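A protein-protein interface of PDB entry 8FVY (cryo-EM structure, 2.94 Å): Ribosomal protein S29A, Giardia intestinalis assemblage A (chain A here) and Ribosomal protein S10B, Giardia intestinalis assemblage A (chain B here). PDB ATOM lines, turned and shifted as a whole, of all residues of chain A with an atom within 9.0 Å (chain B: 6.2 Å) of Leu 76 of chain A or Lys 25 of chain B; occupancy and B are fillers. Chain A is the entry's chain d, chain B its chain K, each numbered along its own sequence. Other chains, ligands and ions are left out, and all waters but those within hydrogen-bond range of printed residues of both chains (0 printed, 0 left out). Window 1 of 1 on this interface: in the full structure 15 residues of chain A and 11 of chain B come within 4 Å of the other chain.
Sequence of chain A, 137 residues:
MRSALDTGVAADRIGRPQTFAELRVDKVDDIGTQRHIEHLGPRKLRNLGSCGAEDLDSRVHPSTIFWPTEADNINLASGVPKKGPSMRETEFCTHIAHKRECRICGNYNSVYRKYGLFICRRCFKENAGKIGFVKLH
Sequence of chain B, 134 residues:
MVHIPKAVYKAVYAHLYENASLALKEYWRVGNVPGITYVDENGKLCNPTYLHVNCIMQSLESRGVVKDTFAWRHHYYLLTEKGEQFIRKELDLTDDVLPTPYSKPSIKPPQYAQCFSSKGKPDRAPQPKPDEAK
OE2 of Glu 101 of chain A lies within salt-bridge range of NE of Arg 73 of chain B (2.7 Å).
A ring nitrogen (NE2) of His 74 of chain B is in hydrogen-bond range of the side-chain amide nitrogen (ND2) of Asn 75 of chain A (3.4 Å).
The side-chain amino group of Lys 25 of chain B sits close to the side-chain amide nitrogen of Asn 75 of chain A, 3.3 Å away.
The backbone carbonyl oxygen (O) of Asn 32 of chain B sits at hydrogen-bond distance from the backbone NH (N) of Ser 78 of chain A (2.8 Å).
O of Asn 75 of chain A is in hydrogen-bond range of OH of Tyr 50 of chain B, 3.2 Å away.
Pro 34 of chain B touches Ile 74 of chain A.
Asn 75 of chain A touches Pro 34 of chain B (O to CD, 3.0 Å).
CG of Lys 25 of chain B touches CB of Leu 76 of chain A (3.6 Å).
Tyr 50 of chain B touches Leu 76 of chain A (OH to CA, 3.3 Å).
Ala 77 of chain A touches Asn 32 of chain B.
CA of Gly 31 of chain B touches O of Gly 79 of chain A (3.8 Å).
Gly 79 of chain A touches Asn 32 of chain B.
Cys 102 of chain A touches Arg 73 of chain B (O to CD, 3.6 Å).
Trp 72 of chain B touches Arg 103 of chain A.
Of chain B, only Lys 25 and Tyr 50 come within 4 Å of Leu 76 of chain A.
Lys 25 of chain B touches just these residues of chain A: Asn 75 and Leu 76.
Printed residues of chain A within 4 Å of Arg 73 of chain B: Glu 101 (2.7 Å) and Cys 102 (3.6 Å).
Of the printed residues of chain B, Glu 101 of chain A touches Arg 73 (2.7 Å).
Of the printed residues of chain A, Gly 31 of chain B touches Gly 79 (3.8 Å).
Of the printed residues of chain B, Ile 74 of chain A touches Pro 34.
Glu 70 of chain A touches none of the printed residues of chain B.
Asp 72 of chain A touches none of the printed residues of chain B.
The nearest residue of chain B that does not touch Leu 76 of chain A is Tyr 27 of chain B (4.1 Å).
The nearest printed residue of chain A that does not touch Arg 73 of chain B is Arg 103 of chain A (4.2 Å).
Of the 14 printed residues of chain B, 8 touch a printed residue of chain A.
Hydrophobic or aromatic side chains of chain B that line the printed part of chain A: Pro 34, Tyr 50, Trp 72 and His 74.
Of the 16 printed residues of chain A, 9 touch a printed residue of chain B.
Along chain A the printed residues that touch a printed residue of chain B span positions 74 to 103.
Among the printed residues, 14 pairs touch across the chains.
Among the printed residues, Asp or Glu carboxylates within 4 Å of a Lys or Arg side-chain nitrogen of the other chain: Glu 101 of chain A with Arg 73 of chain B.
OD1 of Asn 73 of chain A lies within hydrogen-bond range of ND2 of Asn 75 of chain A.
A ring nitrogen (NE2) of His 74 of chain B lies close to the side-chain amino group of Lys 25 of chain B, at 3.1 Å.
The side-chain carboxylate (OD1) of Asp 72 of chain A lies within salt-bridge range of the guanidinium group (NH2) of Arg 103 of chain A, at 3.3 Å.
The backbone NH (N) of Tyr 50 of chain B sits at hydrogen-bond distance from the backbone carbonyl oxygen (O) of Gly 31 of chain B.
A ring nitrogen (ND1) of His 74 of chain B lies within hydrogen-bond range of the backbone carbonyl oxygen (O) of Leu 24 of chain B, at 3.2 Å.
O of Tyr 50 of chain B lies close to OD1 of Asn 54 of chain B (2.5 Å).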
ATOM      1  N   PRO A  68       5.161   8.474 -21.071  1.00  0.00           N
ATOM      2  CA  PRO A  68       6.587   8.814 -20.987  1.00  0.00           C
ATOM      3  C   PRO A  68       7.349   8.082 -19.894  1.00  0.00           C
ATOM      4  O   PRO A  68       8.566   8.250 -19.770  1.00  0.00           O
ATOM      5  CB  PRO A  68       6.548  10.317 -20.696  1.00  0.00           C
ATOM      6  CG  PRO A  68       5.278  10.490 -19.868  1.00  0.00           C
ATOM      7  CD  PRO A  68       4.373   9.294 -20.137  1.00  0.00           C
ATOM      8  N   THR A  69       6.655   7.270 -19.102  1.00  0.00           N
ATOM      9  CA  THR A  69       7.212   6.738 -17.865  1.00  0.00           C
ATOM     10  C   THR A  69       7.517   7.864 -16.885  1.00  0.00           C
ATOM     11  O   THR A  69       7.142   9.017 -17.120  1.00  0.00           O
ATOM     12  CB  THR A  69       8.485   5.934 -18.119  1.00  0.00           C
ATOM     13  OG1 THR A  69       9.588   6.827 -18.292  1.00  0.00           O
ATOM     14  CG2 THR A  69       8.322   5.072 -19.338  1.00  0.00           C
ATOM     15  N   GLU A  70       8.204   7.541 -15.792  1.00  0.00           N
ATOM     16  CA  GLU A  70       8.567   8.523 -14.781  1.00  0.00           C
ATOM     17  C   GLU A  70      10.002   8.279 -14.361  1.00  0.00           C
ATOM     18  O   GLU A  70      10.318   7.225 -13.804  1.00  0.00           O
ATOM     19  CB  GLU A  70       7.650   8.447 -13.560  1.00  0.00           C
ATOM     20  CG  GLU A  70       7.949   9.481 -12.495  1.00  0.00           C
ATOM     21  CD  GLU A  70       8.697   8.926 -11.298  1.00  0.00           C
ATOM     22  OE1 GLU A  70       8.760   7.693 -11.132  1.00  0.00           O
ATOM     23  OE2 GLU A  70       9.231   9.736 -10.517  1.00  0.00           O
ATOM     24  N   ALA A  71      10.861   9.251 -14.624  1.00  0.00           N
ATOM     25  CA  ALA A  71      12.269   9.176 -14.274  1.00  0.00           C
ATOM     26  C   ALA A  71      12.457  10.058 -13.046  1.00  0.00           C
ATOM     27  O   ALA A  71      12.625  11.275 -13.151  1.00  0.00           O
ATOM     28  CB  ALA A  71      13.140   9.608 -15.441  1.00  0.00           C
ATOM     29  N   ASP A  72      12.413   9.429 -11.872  1.00  0.00           N
ATOM     30  CA  ASP A  72      12.524  10.173 -10.624  1.00  0.00           C
ATOM     31  C   ASP A  72      13.827  10.955 -10.568  1.00  0.00           C
ATOM     32  O   ASP A  72      13.923  11.963  -9.862  1.00  0.00           O
ATOM     33  CB  ASP A  72      12.420   9.212  -9.444  1.00  0.00           C
ATOM     34  CG  ASP A  72      12.210   9.922  -8.129  1.00  0.00           C
ATOM     35  OD1 ASP A  72      12.278  11.165  -8.099  1.00  0.00           O
ATOM     36  OD2 ASP A  72      11.958   9.231  -7.125  1.00  0.00           O
ATOM     37  N   ASN A  73      14.831  10.510 -11.310  1.00  0.00           N
ATOM     38  CA  ASN A  73      16.126  11.164 -11.334  1.00  0.00           C
ATOM     39  C   ASN A  73      16.757  10.921 -12.695  1.00  0.00           C
ATOM     40  O   ASN A  73      16.494   9.914 -13.356  1.00  0.00           O
ATOM     41  CB  ASN A  73      17.031  10.654 -10.199  1.00  0.00           C
ATOM     42  CG  ASN A  73      18.316  11.464 -10.042  1.00  0.00           C
ATOM     43  OD1 ASN A  73      19.310  10.949  -9.529  1.00  0.00           O
ATOM     44  ND2 ASN A  73      18.306  12.722 -10.476  1.00  0.00           N
ATOM     45  N   ILE A  74      17.597  11.867 -13.111  1.00  0.00           N
ATOM     46  CA  ILE A  74      18.244  11.752 -14.409  1.00  0.00           C
ATOM     47  C   ILE A  74      19.182  10.553 -14.441  1.00  0.00           C
ATOM     48  O   ILE A  74      19.546  10.068 -15.517  1.00  0.00           O
ATOM     49  CB  ILE A  74      18.986  13.061 -14.754  1.00  0.00           C
ATOM     50  CG1 ILE A  74      18.091  14.279 -14.480  1.00  0.00           C
ATOM     51  CG2 ILE A  74      19.451  13.051 -16.211  1.00  0.00           C
ATOM     52  CD1 ILE A  74      18.753  15.620 -14.754  1.00  0.00           C
ATOM     53  N   ASN A  75      19.586  10.053 -13.273  1.00  0.00           N
ATOM     54  CA  ASN A  75      20.569   8.976 -13.226  1.00  0.00           C
ATOM     55  C   ASN A  75      20.004   7.670 -13.759  1.00  0.00           C
ATOM     56  O   ASN A  75      20.714   6.908 -14.423  1.00  0.00           O
ATOM     57  CB  ASN A  75      21.051   8.763 -11.793  1.00  0.00           C
ATOM     58  CG  ASN A  75      19.922   8.471 -10.851  1.00  0.00           C
ATOM     59  OD1 ASN A  75      18.819   8.130 -11.265  1.00  0.00           O
ATOM     60  ND2 ASN A  75      20.191   8.596  -9.574  1.00  0.00           N
ATOM     61  N   LEU A  76      18.736   7.403 -13.484  1.00  0.00           N
ATOM     62  CA  LEU A  76      18.142   6.089 -13.662  1.00  0.00           C
ATOM     63  C   LEU A  76      17.770   5.776 -15.104  1.00  0.00           C
ATOM     64  O   LEU A  76      17.030   4.818 -15.339  1.00  0.00           O
ATOM     65  CB  LEU A  76      16.920   5.955 -12.742  1.00  0.00           C
ATOM     66  CG  LEU A  76      15.649   6.740 -13.078  1.00  0.00           C
ATOM     67  CD1 LEU A  76      14.596   5.841 -13.688  1.00  0.00           C
ATOM     68  CD2 LEU A  76      15.139   7.430 -11.817  1.00  0.00           C
ATOM     69  N   ALA A  77      18.276   6.542 -16.069  1.00  0.00           N
ATOM     70  CA  ALA A  77      18.120   6.209 -17.477  1.00  0.00           C
ATOM     71  C   ALA A  77      18.597   7.346 -18.362  1.00  0.00           C
ATOM     72  O   ALA A  77      18.832   8.461 -17.887  1.00  0.00           O
ATOM     73  CB  ALA A  77      16.671   5.881 -17.806  1.00  0.00           C
ATOM     74  N   SER A  78      18.735   7.066 -19.657  1.00  0.00           N
ATOM     75  CA  SER A  78      19.090   8.073 -20.647  1.00  0.00           C
ATOM     76  C   SER A  78      18.467   7.636 -21.965  1.00  0.00           C
ATOM     77  O   SER A  78      19.136   7.175 -22.887  1.00  0.00           O
ATOM     78  CB  SER A  78      20.599   8.225 -20.743  1.00  0.00           C
ATOM     79  OG  SER A  78      20.970   9.127 -21.758  1.00  0.00           O
ATOM     80  N   GLY A  79      17.149   7.770 -22.035  1.00  0.00           N
ATOM     81  CA  GLY A  79      16.408   7.409 -23.224  1.00  0.00           C
ATOM     82  C   GLY A  79      16.495   5.926 -23.507  1.00  0.00           C
ATOM     83  O   GLY A  79      17.020   5.167 -22.695  1.00  0.00           O
ATOM     84  N   LYS A  99       5.498   4.104 -14.583  1.00  0.00           N
ATOM     85  CA  LYS A  99       5.920   3.091 -13.633  1.00  0.00           C
ATOM     86  C   LYS A  99       6.324   3.756 -12.338  1.00  0.00           C
ATOM     87  O   LYS A  99       7.263   3.328 -11.661  1.00  0.00           O
ATOM     88  CB  LYS A  99       7.060   2.253 -14.193  1.00  0.00           C
ATOM     89  CG  LYS A  99       6.661   1.388 -15.369  1.00  0.00           C
ATOM     90  CD  LYS A  99       6.041   0.093 -14.907  1.00  0.00           C
ATOM     91  CE  LYS A  99       5.870  -0.881 -16.056  1.00  0.00           C
ATOM     92  NZ  LYS A  99       5.224  -2.142 -15.604  1.00  0.00           N
ATOM     93  N   GLU A 101       6.945   4.793  -8.728  1.00  0.00           N
ATOM     94  CA  GLU A 101       7.127   3.896  -7.604  1.00  0.00           C
ATOM     95  C   GLU A 101       7.785   4.646  -6.462  1.00  0.00           C
ATOM     96  O   GLU A 101       8.400   5.695  -6.655  1.00  0.00           O
ATOM     97  CB  GLU A 101       7.967   2.697  -8.001  1.00  0.00           C
ATOM     98  CG  GLU A 101       9.282   3.067  -8.550  1.00  0.00           C
ATOM     99  CD  GLU A 101      10.362   2.101  -8.155  1.00  0.00           C
ATOM    100  OE1 GLU A 101      10.038   0.913  -7.947  1.00  0.00           O
ATOM    101  OE2 GLU A 101      11.533   2.522  -8.057  1.00  0.00           O
ATOM    102  N   CYS A 102       7.638   4.095  -5.268  1.00  0.00           N
ATOM    103  CA  CYS A 102       8.300   4.643  -4.104  1.00  0.00           C
ATOM    104  C   CYS A 102       9.797   4.664  -4.313  1.00  0.00           C
ATOM    105  O   CYS A 102      10.385   3.694  -4.792  1.00  0.00           O
ATOM    106  CB  CYS A 102       7.953   3.817  -2.875  1.00  0.00           C
ATOM    107  SG  CYS A 102       8.321   4.534  -1.287  1.00  0.00           S
ATOM    108  N   ARG A 103      10.407   5.775  -3.945  1.00  0.00           N
ATOM    109  CA  ARG A 103      11.845   5.916  -3.978  1.00  0.00           C
ATOM    110  C   ARG A 103      12.525   5.359  -2.745  1.00  0.00           C
ATOM    111  O   ARG A 103      13.662   5.728  -2.469  1.00  0.00           O
ATOM    112  CB  ARG A 103      12.215   7.380  -4.175  1.00  0.00           C
ATOM    113  CG  ARG A 103      11.615   8.278  -3.194  1.00  0.00           C
ATOM    114  CD  ARG A 103      12.490   9.440  -2.835  1.00  0.00           C
ATOM    115  NE  ARG A 103      12.847  10.349  -3.910  1.00  0.00           N
ATOM    116  CZ  ARG A 103      12.201  11.469  -4.199  1.00  0.00           C
ATOM    117  NH1 ARG A 103      11.053  11.773  -3.640  1.00  0.00           N
ATOM    118  NH2 ARG A 103      12.724  12.309  -5.078  1.00  0.00           N
ATOM    119  N   ALA B  23      27.812   4.590  -7.747  1.00  0.00           N
ATOM    120  CA  ALA B  23      26.465   4.518  -7.208  1.00  0.00           C
ATOM    121  C   ALA B  23      25.500   4.325  -8.362  1.00  0.00           C
ATOM    122  O   ALA B  23      25.384   5.188  -9.233  1.00  0.00           O
ATOM    123  CB  ALA B  23      26.105   5.767  -6.416  1.00  0.00           C
ATOM    124  N   LEU B  24      24.797   3.205  -8.346  1.00  0.00           N
ATOM    125  CA  LEU B  24      24.051   2.712  -9.484  1.00  0.00           C
ATOM    126  C   LEU B  24      22.617   2.424  -9.085  1.00  0.00           C
ATOM    127  O   LEU B  24      22.350   1.981  -7.967  1.00  0.00           O
ATOM    128  CB  LEU B  24      24.721   1.469 -10.024  1.00  0.00           C
ATOM    129  CG  LEU B  24      24.013   0.681 -11.086  1.00  0.00           C
ATOM    130  CD1 LEU B  24      24.325   1.326 -12.356  1.00  0.00           C
ATOM    131  CD2 LEU B  24      24.483  -0.729 -11.068  1.00  0.00           C
ATOM    132  N   LYS B  25      21.705   2.696 -10.003  1.00  0.00           N
ATOM    133  CA  LYS B  25      20.294   2.440  -9.785  1.00  0.00           C
ATOM    134  C   LYS B  25      19.980   0.958  -9.805  1.00  0.00           C
ATOM    135  O   LYS B  25      20.702   0.154 -10.393  1.00  0.00           O
ATOM    136  CB  LYS B  25      19.475   3.134 -10.853  1.00  0.00           C
ATOM    137  CG  LYS B  25      18.025   3.357 -10.526  1.00  0.00           C
ATOM    138  CD  LYS B  25      17.834   4.139  -9.288  1.00  0.00           C
ATOM    139  CE  LYS B  25      18.678   5.388  -9.276  1.00  0.00           C
ATOM    140  NZ  LYS B  25      18.297   6.340  -8.197  1.00  0.00           N
ATOM    141  N   GLU B  26      18.877   0.610  -9.165  1.00  0.00           N
ATOM    142  CA  GLU B  26      18.320  -0.730  -9.218  1.00  0.00           C
ATOM    143  C   GLU B  26      17.291  -0.732 -10.332  1.00  0.00           C
ATOM    144  O   GLU B  26      16.156  -0.286 -10.148  1.00  0.00           O
ATOM    145  CB  GLU B  26      17.699  -1.101  -7.883  1.00  0.00           C
ATOM    146  CG  GLU B  26      17.884  -2.523  -7.479  1.00  0.00           C
ATOM    147  CD  GLU B  26      17.374  -3.505  -8.508  1.00  0.00           C
ATOM    148  OE1 GLU B  26      16.421  -3.166  -9.235  1.00  0.00           O
ATOM    149  OE2 GLU B  26      17.936  -4.617  -8.591  1.00  0.00           O
ATOM    150  N   TYR B  27      17.685  -1.221 -11.499  1.00  0.00           N
ATOM    151  CA  TYR B  27      16.878  -1.094 -12.693  1.00  0.00           C
ATOM    152  C   TYR B  27      17.156  -2.301 -13.561  1.00  0.00           C
ATOM    153  O   TYR B  27      18.220  -2.915 -13.477  1.00  0.00           O
ATOM    154  CB  TYR B  27      17.198   0.207 -13.408  1.00  0.00           C
ATOM    155  CG  TYR B  27      16.178   0.730 -14.372  1.00  0.00           C
ATOM    156  CD1 TYR B  27      15.054   1.389 -13.928  1.00  0.00           C
ATOM    157  CD2 TYR B  27      16.383   0.640 -15.729  1.00  0.00           C
ATOM    158  CE1 TYR B  27      14.139   1.894 -14.808  1.00  0.00           C
ATOM    159  CE2 TYR B  27      15.480   1.144 -16.610  1.00  0.00           C
ATOM    160  CZ  TYR B  27      14.361   1.772 -16.148  1.00  0.00           C
ATOM    161  OH  TYR B  27      13.457   2.276 -17.045  1.00  0.00           O
ATOM    162  N   GLY B  31      17.567   0.946 -20.628  1.00  0.00           N
ATOM    163  CA  GLY B  31      17.955   2.314 -20.406  1.00  0.00           C
ATOM    164  C   GLY B  31      19.445   2.458 -20.549  1.00  0.00           C
ATOM    165  O   GLY B  31      20.181   1.470 -20.636  1.00  0.00           O
ATOM    166  N   ASN B  32      19.879   3.707 -20.567  1.00  0.00           N
ATOM    167  CA  ASN B  32      21.270   4.059 -20.780  1.00  0.00           C
ATOM    168  C   ASN B  32      21.777   4.808 -19.562  1.00  0.00           C
ATOM    169  O   ASN B  32      21.123   5.736 -19.084  1.00  0.00           O
ATOM    170  CB  ASN B  32      21.420   4.904 -22.040  1.00  0.00           C
ATOM    171  CG  ASN B  32      21.975   4.126 -23.200  1.00  0.00           C
ATOM    172  OD1 ASN B  32      23.180   4.100 -23.413  1.00  0.00           O
ATOM    173  ND2 ASN B  32      21.106   3.485 -23.956  1.00  0.00           N
ATOM    174  N   PRO B  34      23.687   7.515 -17.575  1.00  0.00           N
ATOM    175  CA  PRO B  34      24.104   8.858 -17.969  1.00  0.00           C
ATOM    176  C   PRO B  34      25.496   9.246 -17.512  1.00  0.00           C
ATOM    177  O   PRO B  34      26.018  10.267 -17.977  1.00  0.00           O
ATOM    178  CB  PRO B  34      23.053   9.728 -17.283  1.00  0.00           C
ATOM    179  CG  PRO B  34      22.736   8.994 -16.072  1.00  0.00           C
ATOM    180  CD  PRO B  34      22.909   7.548 -16.331  1.00  0.00           C
ATOM    181  N   TYR B  50      22.034  -0.436 -18.880  1.00  0.00           N
ATOM    182  CA  TYR B  50      21.999  -0.896 -17.506  1.00  0.00           C
ATOM    183  C   TYR B  50      22.315  -2.377 -17.395  1.00  0.00           C
ATOM    184  O   TYR B  50      22.926  -2.816 -16.418  1.00  0.00           O
ATOM    185  CB  TYR B  50      20.632  -0.596 -16.927  1.00  0.00           C
ATOM    186  CG  TYR B  50      20.619   0.580 -16.021  1.00  0.00           C
ATOM    187  CD1 TYR B  50      21.003   0.468 -14.714  1.00  0.00           C
ATOM    188  CD2 TYR B  50      20.213   1.803 -16.474  1.00  0.00           C
ATOM    189  CE1 TYR B  50      20.992   1.541 -13.891  1.00  0.00           C
ATOM    190  CE2 TYR B  50      20.196   2.881 -15.657  1.00  0.00           C
ATOM    191  CZ  TYR B  50      20.587   2.745 -14.365  1.00  0.00           C
ATOM    192  OH  TYR B  50      20.579   3.825 -13.535  1.00  0.00           O
ATOM    193  N   ASN B  54      25.230  -3.910 -14.983  1.00  0.00           N
ATOM    194  CA  ASN B  54      24.744  -4.613 -13.812  1.00  0.00           C
ATOM    195  C   ASN B  54      25.343  -6.004 -13.729  1.00  0.00           C
ATOM    196  O   ASN B  54      25.759  -6.447 -12.652  1.00  0.00           O
ATOM    197  CB  ASN B  54      23.226  -4.655 -13.845  1.00  0.00           C
ATOM    198  CG  ASN B  54      22.610  -3.312 -13.548  1.00  0.00           C
ATOM    199  OD1 ASN B  54      23.117  -2.284 -13.977  1.00  0.00           O
ATOM    200  ND2 ASN B  54      21.530  -3.307 -12.797  1.00  0.00           N
ATOM    201  N   TRP B  72      18.153   3.373  -0.339  1.00  0.00           N
ATOM    202  CA  TRP B  72      16.865   3.718  -0.927  1.00  0.00           C
ATOM    203  C   TRP B  72      16.874   3.309  -2.396  1.00  0.00           C
ATOM    204  O   TRP B  72      16.904   4.122  -3.321  1.00  0.00           O
ATOM    205  CB  TRP B  72      16.581   5.200  -0.791  1.00  0.00           C
ATOM    206  CG  TRP B  72      16.191   5.648   0.502  1.00  0.00           C
ATOM    207  CD1 TRP B  72      16.381   5.030   1.673  1.00  0.00           C
ATOM    208  CD2 TRP B  72      15.537   6.865   0.783  1.00  0.00           C
ATOM    209  NE1 TRP B  72      15.873   5.782   2.684  1.00  0.00           N
ATOM    210  CE2 TRP B  72      15.347   6.923   2.152  1.00  0.00           C
ATOM    211  CE3 TRP B  72      15.087   7.914  -0.003  1.00  0.00           C
ATOM    212  CZ2 TRP B  72      14.731   7.983   2.758  1.00  0.00           C
ATOM    213  CZ3 TRP B  72      14.479   8.955   0.594  1.00  0.00           C
ATOM    214  CH2 TRP B  72      14.300   8.994   1.957  1.00  0.00           C
ATOM    215  N   ARG B  73      16.856   2.006  -2.584  1.00  0.00           N
ATOM    216  CA  ARG B  73      16.891   1.389  -3.895  1.00  0.00           C
ATOM    217  C   ARG B  73      17.953   2.019  -4.791  1.00  0.00           C
ATOM    218  O   ARG B  73      17.710   2.406  -5.932  1.00  0.00           O
ATOM    219  CB  ARG B  73      15.512   1.420  -4.526  1.00  0.00           C
ATOM    220  CG  ARG B  73      15.040   2.676  -5.058  1.00  0.00           C
ATOM    221  CD  ARG B  73      13.646   2.460  -5.580  1.00  0.00           C
ATOM    222  NE  ARG B  73      13.542   1.463  -6.638  1.00  0.00           N
ATOM    223  CZ  ARG B  73      13.432   0.153  -6.444  1.00  0.00           C
ATOM    224  NH1 ARG B  73      13.408  -0.375  -5.234  1.00  0.00           N
ATOM    225  NH2 ARG B  73      13.325  -0.651  -7.492  1.00  0.00           N
ATOM    226  N   HIS B  74      19.168   2.064  -4.259  1.00  0.00           N
ATOM    227  CA  HIS B  74      20.344   2.477  -4.990  1.00  0.00           C
ATOM    228  C   HIS B  74      21.484   1.575  -4.579  1.00  0.00           C
ATOM    229  O   HIS B  74      21.613   1.211  -3.413  1.00  0.00           O
ATOM    230  CB  HIS B  74      20.721   3.907  -4.679  1.00  0.00           C
ATOM    231  CG  HIS B  74      21.138   4.685  -5.868  1.00  0.00           C
ATOM    232  ND1 HIS B  74      22.425   4.697  -6.351  1.00  0.00           N
ATOM    233  CD2 HIS B  74      20.437   5.534  -6.639  1.00  0.00           C
ATOM    234  CE1 HIS B  74      22.483   5.486  -7.406  1.00  0.00           C
ATOM    235  NE2 HIS B  74      21.286   6.007  -7.599  1.00  0.00           N
ATOM    236  N   HIS B  75      22.311   1.218  -5.540  1.00  0.00           N
ATOM    237  CA  HIS B  75      23.491   0.419  -5.287  1.00  0.00           C
ATOM    238  C   HIS B  75      24.681   1.317  -5.064  1.00  0.00           C
ATOM    239  O   HIS B  75      24.978   2.175  -5.896  1.00  0.00           O
ATOM    240  CB  HIS B  75      23.794  -0.500  -6.445  1.00  0.00           C
ATOM    241  CG  HIS B  75      23.120  -1.826  -6.375  1.00  0.00           C
ATOM    242  ND1 HIS B  75      23.402  -2.749  -5.395  1.00  0.00           N
ATOM    243  CD2 HIS B  75      22.224  -2.413  -7.199  1.00  0.00           C
ATOM    244  CE1 HIS B  75      22.681  -3.836  -5.600  1.00  0.00           C
ATOM    245  NE2 HIS B  75      21.961  -3.658  -6.691  1.00  0.00           N
